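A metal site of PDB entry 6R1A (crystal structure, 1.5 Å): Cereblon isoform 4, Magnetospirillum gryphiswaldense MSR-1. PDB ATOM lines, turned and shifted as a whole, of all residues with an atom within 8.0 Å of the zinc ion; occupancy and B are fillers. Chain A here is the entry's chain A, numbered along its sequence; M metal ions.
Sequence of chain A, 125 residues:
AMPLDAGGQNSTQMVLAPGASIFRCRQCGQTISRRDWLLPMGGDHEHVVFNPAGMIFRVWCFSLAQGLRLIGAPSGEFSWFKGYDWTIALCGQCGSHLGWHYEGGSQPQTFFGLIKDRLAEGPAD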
ATOM      1  N   ARG A  24     -10.361  24.320  24.071  1.00  0.00           N
ATOM      2  CA  ARG A  24      -8.948  24.429  24.324  1.00  0.00           C
ATOM      3  C   ARG A  24      -8.426  25.769  23.862  1.00  0.00           C
ATOM      4  O   ARG A  24      -9.043  26.416  23.019  1.00  0.00           O
ATOM      5  CB  ARG A  24      -8.162  23.314  23.602  1.00  0.00           C
ATOM      6  CG  ARG A  24      -8.523  21.932  24.005  1.00  0.00           C
ATOM      7  CD  ARG A  24      -7.778  20.823  23.304  1.00  0.00           C
ATOM      8  NE  ARG A  24      -8.111  19.561  23.942  1.00  0.00           N
ATOM      9  CZ  ARG A  24      -7.669  19.169  25.132  1.00  0.00           C
ATOM     10  NH1 ARG A  24      -6.713  19.838  25.779  1.00  0.00           N
ATOM     11  NH2 ARG A  24      -8.141  18.043  25.654  1.00  0.00           N
ATOM     12  N   CYS A  25      -7.278  26.183  24.382  1.00  0.00           N
ATOM     13  CA  CYS A  25      -6.613  27.353  23.859  1.00  0.00           C
ATOM     14  C   CYS A  25      -6.266  27.133  22.378  1.00  0.00           C
ATOM     15  O   CYS A  25      -5.674  26.108  22.042  1.00  0.00           O
ATOM     16  CB  CYS A  25      -5.392  27.656  24.657  1.00  0.00           C
ATOM     17  SG  CYS A  25      -4.375  29.006  23.968  1.00  0.00           S
ATOM     18  N   ARG A  26      -6.664  28.069  21.536  1.00  0.00           N
ATOM     19  CA  ARG A  26      -6.385  27.986  20.108  1.00  0.00           C
ATOM     20  C   ARG A  26      -4.894  27.970  19.776  1.00  0.00           C
ATOM     21  O   ARG A  26      -4.482  27.389  18.759  1.00  0.00           O
ATOM     22  CB  ARG A  26      -7.079  29.142  19.396  1.00  0.00           C
ATOM     23  CG  ARG A  26      -6.857  29.188  17.917  1.00  0.00           C
ATOM     24  CD  ARG A  26      -7.643  30.317  17.333  1.00  0.00           C
ATOM     25  NE  ARG A  26      -7.305  30.500  15.938  1.00  0.00           N
ATOM     26  CZ  ARG A  26      -7.848  31.406  15.144  1.00  0.00           C
ATOM     27  NH1 ARG A  26      -8.798  32.231  15.579  1.00  0.00           N
ATOM     28  NH2 ARG A  26      -7.417  31.466  13.874  1.00  0.00           N
ATOM     29  N   GLN A  27      -4.099  28.628  20.592  1.00  0.00           N
ATOM     30  CA  GLN A  27      -2.654  28.743  20.308  1.00  0.00           C
ATOM     31  C   GLN A  27      -1.839  27.522  20.716  1.00  0.00           C
ATOM     32  O   GLN A  27      -0.894  27.171  20.050  1.00  0.00           O
ATOM     33  CB  GLN A  27      -2.089  30.017  20.931  1.00  0.00           C
ATOM     34  CG  GLN A  27      -2.779  31.264  20.422  1.00  0.00           C
ATOM     35  CD  GLN A  27      -2.844  31.391  18.896  1.00  0.00           C
ATOM     36  OE1 GLN A  27      -3.877  31.786  18.348  1.00  0.00           O
ATOM     37  NE2 GLN A  27      -1.772  31.076  18.230  1.00  0.00           N
ATOM     38  N   CYS A  28      -2.213  26.841  21.784  1.00  0.00           N
ATOM     39  CA  CYS A  28      -1.413  25.760  22.328  1.00  0.00           C
ATOM     40  C   CYS A  28      -2.125  24.474  22.685  1.00  0.00           C
ATOM     41  O   CYS A  28      -1.474  23.463  22.987  1.00  0.00           O
ATOM     42  CB  CYS A  28      -0.597  26.276  23.506  1.00  0.00           C
ATOM     43  SG  CYS A  28      -1.603  26.480  24.981  1.00  0.00           S
ATOM     44  N   GLY A  29      -3.456  24.480  22.744  1.00  0.00           N
ATOM     45  CA  GLY A  29      -4.190  23.288  23.137  1.00  0.00           C
ATOM     46  C   GLY A  29      -4.480  23.025  24.597  1.00  0.00           C
ATOM     47  O   GLY A  29      -5.127  22.037  24.935  1.00  0.00           O
ATOM     48  N   GLN A  30      -4.051  23.922  25.479  1.00  0.00           N
ATOM     49  CA  GLN A  30      -4.387  23.809  26.894  1.00  0.00           C
ATOM     50  C   GLN A  30      -5.882  23.648  27.071  1.00  0.00           C
ATOM     51  O   GLN A  30      -6.628  24.366  26.479  1.00  0.00           O
ATOM     52  CB  GLN A  30      -3.948  25.075  27.629  1.00  0.00           C
ATOM     53  CG  GLN A  30      -4.368  25.165  29.080  1.00  0.00           C
ATOM     54  CD  GLN A  30      -3.349  24.636  30.028  1.00  0.00           C
ATOM     55  OE1 GLN A  30      -2.838  23.552  29.858  1.00  0.00           O
ATOM     56  NE2 GLN A  30      -3.027  25.430  31.047  1.00  0.00           N
ATOM     57  N   THR A  31      -6.280  22.717  27.927  1.00  0.00           N
ATOM     58  CA  THR A  31      -7.699  22.513  28.246  1.00  0.00           C
ATOM     59  C   THR A  31      -8.225  23.715  29.005  1.00  0.00           C
ATOM     60  O   THR A  31      -7.586  24.075  30.002  1.00  0.00           O
ATOM     61  CB  THR A  31      -7.913  21.262  29.122  1.00  0.00           C
ATOM     62  OG1 THR A  31      -7.142  20.156  28.619  1.00  0.00           O
ATOM     63  CG2 THR A  31      -9.336  20.923  29.118  1.00  0.00           C
ATOM     64  N   ILE A  32      -9.299  24.339  28.556  1.00  0.00           N
ATOM     65  CA  ILE A  32      -9.825  25.554  29.192  1.00  0.00           C
ATOM     66  C   ILE A  32     -11.246  25.405  29.715  1.00  0.00           C
ATOM     67  O   ILE A  32     -11.491  25.737  30.867  1.00  0.00           O
ATOM     68  CB  ILE A  32      -9.794  26.791  28.250  1.00  0.00           C
ATOM     69  CG1 ILE A  32      -8.385  27.059  27.720  1.00  0.00           C
ATOM     70  CG2 ILE A  32     -10.328  28.041  28.944  1.00  0.00           C
ATOM     71  CD1 ILE A  32      -7.340  27.408  28.767  1.00  0.00           C
ATOM     72  N   GLY A  67      -7.054  25.878  33.589  1.00  0.00           N
ATOM     73  CA  GLY A  67      -5.889  26.042  32.721  1.00  0.00           C
ATOM     74  C   GLY A  67      -5.516  27.482  32.440  1.00  0.00           C
ATOM     75  O   GLY A  67      -4.686  27.762  31.574  1.00  0.00           O
ATOM     76  N   LEU A  68      -6.124  28.426  33.145  1.00  0.00           N
ATOM     77  CA  LEU A  68      -5.867  29.848  32.974  1.00  0.00           C
ATOM     78  C   LEU A  68      -4.935  30.287  34.085  1.00  0.00           C
ATOM     79  O   LEU A  68      -4.653  29.526  35.005  1.00  0.00           O
ATOM     80  CB  LEU A  68      -7.163  30.641  33.051  1.00  0.00           C
ATOM     81  CG  LEU A  68      -8.194  30.343  31.940  1.00  0.00           C
ATOM     82  CD1 LEU A  68      -9.590  30.774  32.355  1.00  0.00           C
ATOM     83  CD2 LEU A  68      -7.781  30.868  30.570  1.00  0.00           C
ATOM     84  N   LEU A  90      -5.199  34.755  31.338  1.00  0.00           N
ATOM     85  CA  LEU A  90      -4.299  34.284  30.297  1.00  0.00           C
ATOM     86  C   LEU A  90      -4.362  32.769  30.263  1.00  0.00           C
ATOM     87  O   LEU A  90      -4.631  32.119  31.277  1.00  0.00           O
ATOM     88  CB  LEU A  90      -2.877  34.711  30.565  1.00  0.00           C
ATOM     89  CG  LEU A  90      -2.650  36.198  30.771  1.00  0.00           C
ATOM     90  CD1 LEU A  90      -1.157  36.403  31.051  1.00  0.00           C
ATOM     91  CD2 LEU A  90      -3.186  37.036  29.599  1.00  0.00           C
ATOM     92  N   CYS A  91      -4.100  32.216  29.095  1.00  0.00           N
ATOM     93  CA  CYS A  91      -3.785  30.783  29.027  1.00  0.00           C
ATOM     94  C   CYS A  91      -2.608  30.516  29.954  1.00  0.00           C
ATOM     95  O   CYS A  91      -1.546  31.148  29.854  1.00  0.00           O
ATOM     96  CB  CYS A  91      -3.460  30.373  27.607  1.00  0.00           C
ATOM     97  SG  CYS A  91      -2.996  28.626  27.465  1.00  0.00           S
ATOM     98  N   GLY A  92      -2.782  29.551  30.866  1.00  0.00           N
ATOM     99  CA  GLY A  92      -1.764  29.249  31.844  1.00  0.00           C
ATOM    100  C   GLY A  92      -0.574  28.552  31.253  1.00  0.00           C
ATOM    101  O   GLY A  92       0.459  28.485  31.896  1.00  0.00           O
ATOM    102  N   GLN A  93      -0.720  28.027  30.045  1.00  0.00           N
ATOM    103  CA  GLN A  93       0.348  27.340  29.357  1.00  0.00           C
ATOM    104  C   GLN A  93       1.131  28.327  28.493  1.00  0.00           C
ATOM    105  O   GLN A  93       2.333  28.485  28.667  1.00  0.00           O
ATOM    106  CB  GLN A  93      -0.235  26.170  28.556  1.00  0.00           C
ATOM    107  CG  GLN A  93       0.785  25.327  27.847  1.00  0.00           C
ATOM    108  CD  GLN A  93       0.278  23.953  27.541  1.00  0.00           C
ATOM    109  OE1 GLN A  93       0.471  23.046  28.358  1.00  0.00           O
ATOM    110  NE2 GLN A  93      -0.433  23.786  26.422  1.00  0.00           N
ATOM    111  N   CYS A  94       0.457  29.016  27.568  1.00  0.00           N
ATOM    112  CA  CYS A  94       1.189  29.845  26.588  1.00  0.00           C
ATOM    113  C   CYS A  94       1.111  31.365  26.746  1.00  0.00           C
ATOM    114  O   CYS A  94       1.825  32.090  26.055  1.00  0.00           O
ATOM    115  CB  CYS A  94       0.740  29.481  25.195  1.00  0.00           C
ATOM    116  SG  CYS A  94      -0.843  30.209  24.662  1.00  0.00           S
ATOM    117  N   GLY A  95       0.225  31.836  27.651  1.00  0.00           N
ATOM    118  CA  GLY A  95       0.117  33.252  27.921  1.00  0.00           C
ATOM    119  C   GLY A  95      -0.830  34.017  27.019  1.00  0.00           C
ATOM    120  O   GLY A  95      -0.986  35.237  27.177  1.00  0.00           O
ATOM    121  N   SER A  96      -1.493  33.344  26.094  1.00  0.00           N
ATOM    122  CA  SER A  96      -2.485  33.973  25.197  1.00  0.00           C
ATOM    123  C   SER A  96      -3.591  34.580  26.073  1.00  0.00           C
ATOM    124  O   SER A  96      -4.044  33.980  27.049  1.00  0.00           O
ATOM    125  CB  SER A  96      -3.112  32.935  24.263  1.00  0.00           C
ATOM    126  OG  SER A  96      -4.111  33.489  23.433  1.00  0.00           O
ATOM    127  N   HIS A  97      -4.010  35.799  25.716  1.00  0.00           N
ATOM    128  CA  HIS A  97      -5.089  36.415  26.482  1.00  0.00           C
ATOM    129  C   HIS A  97      -6.413  35.823  26.055  1.00  0.00           C
ATOM    130  O   HIS A  97      -6.883  36.088  24.937  1.00  0.00           O
ATOM    131  CB  HIS A  97      -5.078  37.925  26.277  1.00  0.00           C
ATOM    132  CG  HIS A  97      -6.208  38.602  26.952  1.00  0.00           C
ATOM    133  ND1 HIS A  97      -6.765  39.775  26.491  1.00  0.00           N
ATOM    134  CD2 HIS A  97      -6.921  38.260  28.060  1.00  0.00           C
ATOM    135  CE1 HIS A  97      -7.747  40.124  27.293  1.00  0.00           C
ATOM    136  NE2 HIS A  97      -7.874  39.221  28.244  1.00  0.00           N
ATOM    137  N   LEU A  98      -7.024  35.001  26.908  1.00  0.00           N
ATOM    138  CA  LEU A  98      -8.232  34.277  26.547  1.00  0.00           C
ATOM    139  C   LEU A  98      -9.511  34.928  27.023  1.00  0.00           C
ATOM    140  O   LEU A  98     -10.580  34.622  26.511  1.00  0.00           O
ATOM    141  CB  LEU A  98      -8.165  32.837  27.059  1.00  0.00           C
ATOM    142  CG  LEU A  98      -7.059  31.979  26.450  1.00  0.00           C
ATOM    143  CD1 LEU A  98      -7.238  30.533  26.894  1.00  0.00           C
ATOM    144  CD2 LEU A  98      -6.995  32.044  24.913  1.00  0.00           C
ATOM    145  N   ARG A 118     -10.635  32.841  20.327  1.00  0.00           N
ATOM    146  CA  ARG A 118      -9.343  32.467  20.843  1.00  0.00           C
ATOM    147  C   ARG A 118      -9.338  31.066  21.438  1.00  0.00           C
ATOM    148  O   ARG A 118      -8.308  30.615  22.001  1.00  0.00           O
ATOM    149  CB  ARG A 118      -8.879  33.514  21.853  1.00  0.00           C
ATOM    150  CG  ARG A 118      -8.767  34.880  21.179  1.00  0.00           C
ATOM    151  CD  ARG A 118      -8.088  35.896  22.061  1.00  0.00           C
ATOM    152  NE  ARG A 118      -8.138  37.215  21.440  1.00  0.00           N
ATOM    153  CZ  ARG A 118      -7.620  38.332  21.965  1.00  0.00           C
ATOM    154  NH1 ARG A 118      -6.949  38.304  23.132  1.00  0.00           N
ATOM    155  NH2 ARG A 118      -7.758  39.496  21.315  1.00  0.00           N
HETATM  156 ZN    ZN M   1      -2.439  28.631  25.186  1.00  0.00          ZN
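N of Ser 96 lies close to SG of Cys 94, 3.5 Å away.
SG of Cys 28 sits close to N of Gln 30.
SG of Cys 28 sits close to NE2 of Gln 93, 3.3 Å away.
The side-chain sulfur (SG) of Cys 25 lies close to the backbone NH (N) of Gln 27.
The backbone NH (N) of Cys 25 lies within hydrogen-bond range of the backbone carbonyl oxygen (O) of Gln 30 (2.8 Å).
O of Ser 96 lies within hydrogen-bond range of N of Cys 91, 2.7 Å away.
The side-chain sulfur (SG) of Cys 91 sits close to the backbone NH (N) of Gln 93 (3.5 Å).
The zinc ion is bound by SG of Cys 94 (2.3 Å), SG of Cys 28 (2.3 Å), SG of Cys 25 (2.3 Å) and SG of Cys 91 (2.3 Å).
Four residues have an atom within 4 Å of the zinc ion: Cys 25, Cys 28, Cys 91 and Cys 94.
The nearest printed residue that does not touch the zinc ion is Ser 96 (4.5 Å).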
